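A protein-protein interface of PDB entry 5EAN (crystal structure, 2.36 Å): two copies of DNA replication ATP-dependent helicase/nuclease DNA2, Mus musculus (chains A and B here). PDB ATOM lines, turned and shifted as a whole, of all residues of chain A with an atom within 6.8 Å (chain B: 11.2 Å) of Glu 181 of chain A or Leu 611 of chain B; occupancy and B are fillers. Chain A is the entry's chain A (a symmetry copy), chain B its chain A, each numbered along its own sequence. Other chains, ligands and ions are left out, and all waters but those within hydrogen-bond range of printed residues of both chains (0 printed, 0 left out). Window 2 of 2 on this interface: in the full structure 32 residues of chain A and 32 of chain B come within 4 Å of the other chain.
Hydrophobic or aromatic side chains of chain B that line the printed part of chain A: Ile 608 and Leu 611.
Hydrophobic or aromatic side chains of chain A within 4 Å of the printed part of chain B: Leu 188.
No position is printed for both chains.
Of the 7 pairs that touch across the chains among the printed residues, none has its exchanged pair printed and touching as well.
O of Ser 612 of chain B lies within hydrogen-bond range of NZ of Lys 620 of chain B, at 2.9 Å.
N of Ile 608 of chain B is in hydrogen-bond range of O of Leu 643 of chain B.
Leu 611 of chain B touches just these residues of chain A: Glu 181 (3.6 Å), Gln 184 (3.7 Å) and Glu 185 (3.8 Å).
No residue of chain B comes within 4 Å of Ala 179 of chain A.
No residue of chain B comes within 4 Å of Pro 180 of chain A.
No residue of chain B comes within 4 Å of Leu 183 of chain A.
Gln 184 of chain A touches just these residues of chain B: Ile 608 and Leu 611.
Glu 185 of chain A touches just these residues of chain B: Leu 611 (3.8 Å), Ser 612 (3.7 Å) and Ser 613 (2.2 Å).
Printed residues of chain B within 4 Å of Leu 188 of chain A: Ser 613.
Of the printed residues of chain A, Ser 612 of chain B touches Glu 185 (3.7 Å).
Of the printed residues of chain A, Ser 613 of chain B touches Glu 185 and Leu 188.
Of the printed residues of chain A, Ile 608 of chain B touches Gln 184.
The nearest residue of chain B that does not touch Glu 181 of chain A is Tyr 610 of chain B (7.1 Å).
The nearest residue of chain A that does not touch Leu 611 of chain B is Leu 188 of chain A (4.4 Å).
The nearest printed residue of chain A that does not touch Ile 608 of chain B is Leu 188 of chain A (4.4 Å).
The side-chain hydroxyl of Ser 613 of chain B lies close to the side-chain carboxylate of Glu 185 of chain A.
Among the printed residues, merely in contact across the chains: Glu 181 of chain A with Leu 611 of chain B (3.6 Å), Gln 184 of chain A with Ile 608 of chain B (3.8 Å), Gln 184 of chain A with Leu 611 of chain B (3.7 Å), Glu 185 of chain A with Leu 611 of chain B (3.8 Å), Glu 185 of chain A with Ser 612 of chain B (3.7 Å) and Leu 188 of chain A with Ser 613 of chain B (3.4 Å).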
ATOM      1  N   SER A 177      17.715  -8.152  10.463  1.00  0.00           N
ATOM      2  CA  SER A 177      18.858  -7.382  10.013  1.00  0.00           C
ATOM      3  C   SER A 177      19.002  -7.413   8.496  1.00  0.00           C
ATOM      4  O   SER A 177      18.677  -8.400   7.868  1.00  0.00           O
ATOM      5  CB  SER A 177      20.113  -7.984  10.653  1.00  0.00           C
ATOM      6  OG  SER A 177      21.277  -7.722   9.887  1.00  0.00           O
ATOM      7  N   PHE A 178      19.561  -6.362   7.920  1.00  0.00           N
ATOM      8  CA  PHE A 178      19.942  -6.388   6.508  1.00  0.00           C
ATOM      9  C   PHE A 178      21.452  -6.599   6.240  1.00  0.00           C
ATOM     10  O   PHE A 178      21.909  -6.389   5.100  1.00  0.00           O
ATOM     11  CB  PHE A 178      19.466  -5.117   5.809  1.00  0.00           C
ATOM     12  CG  PHE A 178      17.991  -5.054   5.601  1.00  0.00           C
ATOM     13  CD1 PHE A 178      17.159  -4.533   6.584  1.00  0.00           C
ATOM     14  CD2 PHE A 178      17.428  -5.482   4.391  1.00  0.00           C
ATOM     15  CE1 PHE A 178      15.776  -4.458   6.377  1.00  0.00           C
ATOM     16  CE2 PHE A 178      16.060  -5.417   4.181  1.00  0.00           C
ATOM     17  CZ  PHE A 178      15.221  -4.907   5.179  1.00  0.00           C
ATOM     18  N   ALA A 179      22.209  -7.009   7.264  1.00  0.00           N
ATOM     19  CA  ALA A 179      23.617  -7.428   7.097  1.00  0.00           C
ATOM     20  C   ALA A 179      23.711  -8.486   5.989  1.00  0.00           C
ATOM     21  O   ALA A 179      22.932  -9.437   5.989  1.00  0.00           O
ATOM     22  CB  ALA A 179      24.179  -7.986   8.406  1.00  0.00           C
ATOM     23  N   PRO A 180      24.655  -8.322   5.038  1.00  0.00           N
ATOM     24  CA  PRO A 180      24.773  -9.258   3.901  1.00  0.00           C
ATOM     25  C   PRO A 180      24.780 -10.724   4.309  1.00  0.00           C
ATOM     26  O   PRO A 180      24.073 -11.513   3.715  1.00  0.00           O
ATOM     27  CB  PRO A 180      26.109  -8.867   3.244  1.00  0.00           C
ATOM     28  CG  PRO A 180      26.309  -7.447   3.643  1.00  0.00           C
ATOM     29  CD  PRO A 180      25.748  -7.328   5.037  1.00  0.00           C
ATOM     30  N   GLU A 181      25.536 -11.083   5.332  1.00  0.00           N
ATOM     31  CA  GLU A 181      25.591 -12.467   5.788  1.00  0.00           C
ATOM     32  C   GLU A 181      24.235 -12.967   6.280  1.00  0.00           C
ATOM     33  O   GLU A 181      23.908 -14.117   6.051  1.00  0.00           O
ATOM     34  CB  GLU A 181      26.715 -12.695   6.814  1.00  0.00           C
ATOM     35  CG  GLU A 181      26.499 -12.118   8.215  1.00  0.00           C
ATOM     36  CD  GLU A 181      26.805 -10.616   8.360  1.00  0.00           C
ATOM     37  OE1 GLU A 181      26.780  -9.843   7.354  1.00  0.00           O
ATOM     38  OE2 GLU A 181      27.061 -10.193   9.517  1.00  0.00           O
ATOM     39  N   ARG A 182      23.440 -12.104   6.924  1.00  0.00           N
ATOM     40  CA  ARG A 182      22.091 -12.476   7.370  1.00  0.00           C
ATOM     41  C   ARG A 182      21.139 -12.665   6.208  1.00  0.00           C
ATOM     42  O   ARG A 182      20.346 -13.617   6.197  1.00  0.00           O
ATOM     43  CB  ARG A 182      21.545 -11.469   8.365  1.00  0.00           C
ATOM     44  CG  ARG A 182      21.881 -11.824   9.807  1.00  0.00           C
ATOM     45  CD  ARG A 182      20.657 -12.390  10.545  1.00  0.00           C
ATOM     46  NE  ARG A 182      20.888 -12.640  11.987  1.00  0.00           N
ATOM     47  CZ  ARG A 182      21.107 -11.714  12.935  1.00  0.00           C
ATOM     48  NH1 ARG A 182      21.174 -10.420  12.646  1.00  0.00           N
ATOM     49  NH2 ARG A 182      21.288 -12.091  14.201  1.00  0.00           N
ATOM     50  N   LEU A 183      21.245 -11.802   5.201  1.00  0.00           N
ATOM     51  CA  LEU A 183      20.444 -11.947   4.006  1.00  0.00           C
ATOM     52  C   LEU A 183      20.738 -13.272   3.316  1.00  0.00           C
ATOM     53  O   LEU A 183      19.805 -14.000   2.934  1.00  0.00           O
ATOM     54  CB  LEU A 183      20.666 -10.765   3.065  1.00  0.00           C
ATOM     55  CG  LEU A 183      20.271  -9.396   3.616  1.00  0.00           C
ATOM     56  CD1 LEU A 183      20.553  -8.313   2.591  1.00  0.00           C
ATOM     57  CD2 LEU A 183      18.796  -9.372   4.040  1.00  0.00           C
ATOM     58  N   GLN A 184      22.024 -13.606   3.211  1.00  0.00           N
ATOM     59  CA  GLN A 184      22.438 -14.831   2.554  1.00  0.00           C
ATOM     60  C   GLN A 184      21.871 -16.016   3.334  1.00  0.00           C
ATOM     61  O   GLN A 184      21.280 -16.913   2.735  1.00  0.00           O
ATOM     62  CB  GLN A 184      23.960 -14.885   2.381  1.00  0.00           C
ATOM     63  CG  GLN A 184      24.470 -16.146   1.704  1.00  0.00           C
ATOM     64  CD  GLN A 184      24.173 -16.235   0.210  1.00  0.00           C
ATOM     65  OE1 GLN A 184      24.703 -15.464  -0.582  1.00  0.00           O
ATOM     66  NE2 GLN A 184      23.343 -17.207  -0.183  1.00  0.00           N
ATOM     67  N   GLU A 185      21.997 -15.980   4.664  1.00  0.00           N
ATOM     68  CA  GLU A 185      21.303 -16.905   5.552  1.00  0.00           C
ATOM     69  C   GLU A 185      19.790 -17.056   5.281  1.00  0.00           C
ATOM     70  O   GLU A 185      19.298 -18.164   5.064  1.00  0.00           O
ATOM     71  CB  GLU A 185      21.536 -16.506   6.990  1.00  0.00           C
ATOM     72  CG  GLU A 185      22.787 -17.136   7.569  1.00  0.00           C
ATOM     73  CD  GLU A 185      22.501 -18.508   8.142  1.00  0.00           C
ATOM     74  OE1 GLU A 185      23.406 -19.118   8.777  1.00  0.00           O
ATOM     75  OE2 GLU A 185      21.342 -18.970   7.946  1.00  0.00           O
ATOM     76  N   LEU A 186      19.074 -15.938   5.273  1.00  0.00           N
ATOM     77  CA  LEU A 186      17.650 -15.940   4.987  1.00  0.00           C
ATOM     78  C   LEU A 186      17.325 -16.548   3.615  1.00  0.00           C
ATOM     79  O   LEU A 186      16.387 -17.357   3.513  1.00  0.00           O
ATOM     80  CB  LEU A 186      17.103 -14.516   5.082  1.00  0.00           C
ATOM     81  CG  LEU A 186      16.616 -13.912   6.409  1.00  0.00           C
ATOM     82  CD1 LEU A 186      16.938 -14.730   7.649  1.00  0.00           C
ATOM     83  CD2 LEU A 186      17.090 -12.468   6.566  1.00  0.00           C
ATOM     84  N   LEU A 188      19.255 -18.754   1.893  1.00  0.00           N
ATOM     85  CA  LEU A 188      19.512 -20.188   1.995  1.00  0.00           C
ATOM     86  C   LEU A 188      18.346 -20.940   2.659  1.00  0.00           C
ATOM     87  O   LEU A 188      17.912 -21.977   2.166  1.00  0.00           O
ATOM     88  CB  LEU A 188      20.808 -20.470   2.752  1.00  0.00           C
ATOM     89  CG  LEU A 188      22.198 -20.734   2.152  1.00  0.00           C
ATOM     90  CD1 LEU A 188      22.210 -21.066   0.672  1.00  0.00           C
ATOM     91  CD2 LEU A 188      23.231 -19.664   2.500  1.00  0.00           C
ATOM     92  N   PHE B 607      31.579 -18.302  -5.887  1.00  0.00           N
ATOM     93  CA  PHE B 607      31.554 -19.071  -4.626  1.00  0.00           C
ATOM     94  C   PHE B 607      31.075 -18.180  -3.508  1.00  0.00           C
ATOM     95  O   PHE B 607      31.456 -17.023  -3.443  1.00  0.00           O
ATOM     96  CB  PHE B 607      32.966 -19.581  -4.261  1.00  0.00           C
ATOM     97  CG  PHE B 607      33.592 -20.411  -5.342  1.00  0.00           C
ATOM     98  CD1 PHE B 607      34.304 -19.809  -6.380  1.00  0.00           C
ATOM     99  CD2 PHE B 607      33.430 -21.790  -5.352  1.00  0.00           C
ATOM    100  CE1 PHE B 607      34.865 -20.569  -7.387  1.00  0.00           C
ATOM    101  CE2 PHE B 607      33.986 -22.571  -6.367  1.00  0.00           C
ATOM    102  CZ  PHE B 607      34.707 -21.959  -7.386  1.00  0.00           C
ATOM    103  N   ILE B 608      30.249 -18.696  -2.619  1.00  0.00           N
ATOM    104  CA  ILE B 608      29.841 -17.879  -1.469  1.00  0.00           C
ATOM    105  C   ILE B 608      30.782 -18.179  -0.309  1.00  0.00           C
ATOM    106  O   ILE B 608      31.471 -19.195  -0.359  1.00  0.00           O
ATOM    107  CB  ILE B 608      28.354 -18.085  -1.102  1.00  0.00           C
ATOM    108  CG1 ILE B 608      27.997 -19.566  -0.947  1.00  0.00           C
ATOM    109  CG2 ILE B 608      27.492 -17.481  -2.177  1.00  0.00           C
ATOM    110  CD1 ILE B 608      26.861 -19.843   0.020  1.00  0.00           C
ATOM    111  N   ALA B 609      30.806 -17.311   0.709  1.00  0.00           N
ATOM    112  CA  ALA B 609      31.466 -17.568   2.018  1.00  0.00           C
ATOM    113  C   ALA B 609      30.677 -18.589   2.814  1.00  0.00           C
ATOM    114  O   ALA B 609      29.466 -18.629   2.706  1.00  0.00           O
ATOM    115  CB  ALA B 609      31.574 -16.292   2.810  1.00  0.00           C
ATOM    116  N   TYR B 610      31.349 -19.410   3.617  1.00  0.00           N
ATOM    117  CA  TYR B 610      30.692 -20.476   4.373  1.00  0.00           C
ATOM    118  C   TYR B 610      29.782 -19.869   5.424  1.00  0.00           C
ATOM    119  O   TYR B 610      30.114 -18.840   5.957  1.00  0.00           O
ATOM    120  CB  TYR B 610      31.711 -21.425   5.061  1.00  0.00           C
ATOM    121  CG  TYR B 610      30.981 -22.474   5.884  1.00  0.00           C
ATOM    122  CD1 TYR B 610      30.306 -23.514   5.249  1.00  0.00           C
ATOM    123  CD2 TYR B 610      30.880 -22.369   7.285  1.00  0.00           C
ATOM    124  CE1 TYR B 610      29.563 -24.443   5.970  1.00  0.00           C
ATOM    125  CE2 TYR B 610      30.151 -23.303   8.025  1.00  0.00           C
ATOM    126  CZ  TYR B 610      29.499 -24.348   7.354  1.00  0.00           C
ATOM    127  OH  TYR B 610      28.777 -25.305   8.037  1.00  0.00           O
ATOM    128  N   LEU B 611      28.649 -20.519   5.710  1.00  0.00           N
ATOM    129  CA  LEU B 611      27.705 -20.114   6.753  1.00  0.00           C
ATOM    130  C   LEU B 611      27.020 -21.374   7.274  1.00  0.00           C
ATOM    131  O   LEU B 611      26.886 -22.347   6.497  1.00  0.00           O
ATOM    132  CB  LEU B 611      26.629 -19.175   6.181  1.00  0.00           C
ATOM    133  CG  LEU B 611      26.945 -17.781   5.600  1.00  0.00           C
ATOM    134  CD1 LEU B 611      25.679 -17.121   5.078  1.00  0.00           C
ATOM    135  CD2 LEU B 611      27.601 -16.859   6.611  1.00  0.00           C
ATOM    136  N   SER B 612      26.578 -21.370   8.551  1.00  0.00           N
ATOM    137  CA  SER B 612      25.792 -22.494   9.121  1.00  0.00           C
ATOM    138  C   SER B 612      24.743 -23.077   8.170  1.00  0.00           C
ATOM    139  O   SER B 612      24.567 -24.299   8.095  1.00  0.00           O
ATOM    140  CB  SER B 612      25.036 -22.075  10.372  1.00  0.00           C
ATOM    141  OG  SER B 612      25.890 -21.892  11.464  1.00  0.00           O
ATOM    142  N   SER B 613      24.058 -22.198   7.440  1.00  0.00           N
ATOM    143  CA  SER B 613      22.915 -22.612   6.661  1.00  0.00           C
ATOM    144  C   SER B 613      23.239 -23.055   5.269  1.00  0.00           C
ATOM    145  O   SER B 613      22.321 -23.248   4.474  1.00  0.00           O
ATOM    146  CB  SER B 613      21.911 -21.488   6.606  1.00  0.00           C
ATOM    147  OG  SER B 613      21.540 -21.168   7.925  1.00  0.00           O
ATOM    148  N   VAL B 614      24.522 -23.224   4.952  1.00  0.00           N
ATOM    149  CA  VAL B 614      24.868 -23.711   3.628  1.00  0.00           C
ATOM    150  C   VAL B 614      24.282 -25.105   3.355  1.00  0.00           C
ATOM    151  O   VAL B 614      23.768 -25.353   2.259  1.00  0.00           O
ATOM    152  CB  VAL B 614      26.370 -23.620   3.308  1.00  0.00           C
ATOM    153  CG1 VAL B 614      26.674 -24.282   1.971  1.00  0.00           C
ATOM    154  CG2 VAL B 614      26.784 -22.160   3.223  1.00  0.00           C
ATOM    155  N   LEU B 615      24.326 -25.987   4.351  1.00  0.00           N
ATOM    156  CA  LEU B 615      23.758 -27.332   4.196  1.00  0.00           C
ATOM    157  C   LEU B 615      22.463 -27.380   4.943  1.00  0.00           C
ATOM    158  O   LEU B 615      22.362 -26.735   5.992  1.00  0.00           O
ATOM    159  CB  LEU B 615      24.683 -28.397   4.765  1.00  0.00           C
ATOM    160  CG  LEU B 615      26.028 -28.620   4.082  1.00  0.00           C
ATOM    161  CD1 LEU B 615      27.057 -27.562   4.486  1.00  0.00           C
ATOM    162  CD2 LEU B 615      26.558 -29.999   4.439  1.00  0.00           C
ATOM    163  N   PRO B 616      21.463 -28.146   4.426  1.00  0.00           N
ATOM    164  CA  PRO B 616      20.219 -28.388   5.193  1.00  0.00           C
ATOM    165  C   PRO B 616      20.547 -28.866   6.613  1.00  0.00           C
ATOM    166  O   PRO B 616      21.378 -29.743   6.774  1.00  0.00           O
ATOM    167  CB  PRO B 616      19.545 -29.520   4.421  1.00  0.00           C
ATOM    168  CG  PRO B 616      20.070 -29.389   3.039  1.00  0.00           C
ATOM    169  CD  PRO B 616      21.474 -28.889   3.148  1.00  0.00           C
ATOM    170  N   HIS B 617      19.921 -28.281   7.614  1.00  0.00           N
ATOM    171  CA  HIS B 617      20.269 -28.585   8.998  1.00  0.00           C
ATOM    172  C   HIS B 617      20.393 -30.080   9.334  1.00  0.00           C
ATOM    173  O   HIS B 617      21.324 -30.493  10.014  1.00  0.00           O
ATOM    174  CB  HIS B 617      19.312 -27.920   9.983  1.00  0.00           C
ATOM    175  CG  HIS B 617      19.748 -28.076  11.403  1.00  0.00           C
ATOM    176  ND1 HIS B 617      19.217 -29.034  12.248  1.00  0.00           N
ATOM    177  CD2 HIS B 617      20.706 -27.435  12.116  1.00  0.00           C
ATOM    178  CE1 HIS B 617      19.802 -28.952  13.431  1.00  0.00           C
ATOM    179  NE2 HIS B 617      20.710 -27.992  13.377  1.00  0.00           N
ATOM    180  N   LYS B 620      23.768 -31.970   8.407  1.00  0.00           N
ATOM    181  CA  LYS B 620      25.053 -31.479   8.921  1.00  0.00           C
ATOM    182  C   LYS B 620      25.870 -32.553   9.634  1.00  0.00           C
ATOM    183  O   LYS B 620      27.063 -32.688   9.377  1.00  0.00           O
ATOM    184  CB  LYS B 620      24.879 -30.224   9.793  1.00  0.00           C
ATOM    185  CG  LYS B 620      24.182 -29.072   9.056  1.00  0.00           C
ATOM    186  CD  LYS B 620      24.114 -27.774   9.851  1.00  0.00           C
ATOM    187  CE  LYS B 620      25.408 -26.987   9.755  1.00  0.00           C
ATOM    188  NZ  LYS B 620      25.328 -25.712  10.523  1.00  0.00           N
ATOM    189  N   VAL B 623      27.239 -35.350   7.204  1.00  0.00           N
ATOM    190  CA  VAL B 623      28.347 -34.762   6.457  1.00  0.00           C
ATOM    191  C   VAL B 623      29.614 -34.616   7.305  1.00  0.00           C
ATOM    192  O   VAL B 623      30.718 -34.834   6.806  1.00  0.00           O
ATOM    193  CB  VAL B 623      27.960 -33.407   5.831  1.00  0.00           C
ATOM    194  CG1 VAL B 623      29.149 -32.808   5.076  1.00  0.00           C
ATOM    195  CG2 VAL B 623      26.803 -33.604   4.874  1.00  0.00           C
ATOM    196  N   LEU B 627      33.357 -36.041   6.407  1.00  0.00           N
ATOM    197  CA  LEU B 627      34.521 -35.147   6.425  1.00  0.00           C
ATOM    198  C   LEU B 627      35.632 -35.590   7.349  1.00  0.00           C
ATOM    199  O   LEU B 627      36.797 -35.460   6.965  1.00  0.00           O
ATOM    200  CB  LEU B 627      34.122 -33.736   6.820  1.00  0.00           C
ATOM    201  CG  LEU B 627      33.424 -32.840   5.801  1.00  0.00           C
ATOM    202  CD1 LEU B 627      33.312 -31.443   6.408  1.00  0.00           C
ATOM    203  CD2 LEU B 627      34.136 -32.775   4.451  1.00  0.00           C
ATOM    204  N   LYS B 639      34.374 -28.647   0.519  1.00  0.00           N
ATOM    205  CA  LYS B 639      33.955 -27.301   0.867  1.00  0.00           C
ATOM    206  C   LYS B 639      33.769 -26.436  -0.387  1.00  0.00           C
ATOM    207  O   LYS B 639      32.736 -25.798  -0.544  1.00  0.00           O
ATOM    208  CB  LYS B 639      34.993 -26.669   1.781  1.00  0.00           C
ATOM    209  CG  LYS B 639      34.604 -25.317   2.316  1.00  0.00           C
ATOM    210  CD  LYS B 639      35.758 -24.705   3.094  1.00  0.00           C
ATOM    211  CE  LYS B 639      35.459 -23.260   3.397  1.00  0.00           C
ATOM    212  NZ  LYS B 639      36.332 -22.751   4.475  1.00  0.00           N
ATOM    213  N   ARG B 640      34.749 -26.447  -1.281  1.00  0.00           N
ATOM    214  CA  ARG B 640      34.685 -25.656  -2.503  1.00  0.00           C
ATOM    215  C   ARG B 640      33.448 -25.979  -3.332  1.00  0.00           C
ATOM    216  O   ARG B 640      32.771 -25.059  -3.833  1.00  0.00           O
ATOM    217  CB  ARG B 640      35.953 -25.811  -3.351  1.00  0.00           C
ATOM    218  CG  ARG B 640      36.105 -24.747  -4.444  1.00  0.00           C
ATOM    219  CD  ARG B 640      36.407 -23.319  -3.962  1.00  0.00           C
ATOM    220  NE  ARG B 640      37.522 -23.398  -3.034  1.00  0.00           N
ATOM    221  CZ  ARG B 640      38.795 -23.435  -3.411  1.00  0.00           C
ATOM    222  NH1 ARG B 640      39.122 -23.333  -4.718  1.00  0.00           N
ATOM    223  NH2 ARG B 640      39.727 -23.560  -2.488  1.00  0.00           N
ATOM    224  N   LEU B 642      30.577 -27.342  -2.216  1.00  0.00           N
ATOM    225  CA  LEU B 642      29.387 -26.894  -1.500  1.00  0.00           C
ATOM    226  C   LEU B 642      29.164 -25.371  -1.587  1.00  0.00           C
ATOM    227  O   LEU B 642      28.037 -24.883  -1.433  1.00  0.00           O
ATOM    228  CB  LEU B 642      29.472 -27.358  -0.036  1.00  0.00           C
ATOM    229  CG  LEU B 642      29.338 -28.878   0.187  1.00  0.00           C
ATOM    230  CD1 LEU B 642      29.778 -29.274   1.591  1.00  0.00           C
ATOM    231  CD2 LEU B 642      27.915 -29.393  -0.109  1.00  0.00           C
ATOM    232  N   LEU B 643      30.245 -24.624  -1.794  1.00  0.00           N
ATOM    233  CA  LEU B 643      30.166 -23.173  -1.842  1.00  0.00           C
ATOM    234  C   LEU B 643      30.018 -22.627  -3.276  1.00  0.00           C
ATOM    235  O   LEU B 643      29.773 -21.426  -3.471  1.00  0.00           O
ATOM    236  CB  LEU B 643      31.366 -22.542  -1.131  1.00  0.00           C
ATOM    237  CG  LEU B 643      31.522 -22.837   0.380  1.00  0.00           C
ATOM    238  CD1 LEU B 643      32.787 -22.161   0.947  1.00  0.00           C
ATOM    239  CD2 LEU B 643      30.272 -22.518   1.231  1.00  0.00           C
ATOM    240  N   SER B 644      30.139 -23.501  -4.273  1.00  0.00           N
ATOM    241  CA  SER B 644      30.143 -23.076  -5.679  1.00  0.00           C
ATOM    242  C   SER B 644      28.776 -22.656  -6.192  1.00  0.00           C
ATOM    243  O   SER B 644      27.768 -23.145  -5.700  1.00  0.00           O
ATOM    244  CB  SER B 644      30.666 -24.226  -6.537  1.00  0.00           C
ATOM    245  OG  SER B 644      29.744 -25.290  -6.540  1.00  0.00           O
ATOM    246  N   LYS B 645      28.745 -21.767  -7.180  1.00  0.00           N
ATOM    247  CA  LYS B 645      27.515 -21.484  -7.974  1.00  0.00           C
ATOM    248  C   LYS B 645      27.663 -21.982  -9.408  1.00  0.00           C
ATOM    249  O   LYS B 645      26.703 -21.934 -10.196  1.00  0.00           O
ATOM    250  CB  LYS B 645      27.215 -19.991  -8.051  1.00  0.00           C
ATOM    251  CG  LYS B 645      27.255 -19.257  -6.726  1.00  0.00           C
ATOM    252  CD  LYS B 645      26.561 -17.918  -6.873  1.00  0.00           C
ATOM    253  CE  LYS B 645      26.650 -17.215  -5.548  1.00  0.00           C
ATOM    254  NZ  LYS B 645      25.672 -16.125  -5.445  1.00  0.00           N
ATOM    255  N   CYS B 672      22.918 -34.406   1.432  1.00  0.00           N
ATOM    256  CA  CYS B 672      22.349 -33.062   1.341  1.00  0.00           C
ATOM    257  C   CYS B 672      21.079 -33.076   0.521  1.00  0.00           C
ATOM    258  O   CYS B 672      20.419 -32.059   0.401  1.00  0.00           O
ATOM    259  CB  CYS B 672      23.337 -32.068   0.730  1.00  0.00           C
ATOM    260  SG  CYS B 672      24.693 -31.583   1.821  1.00  0.00           S
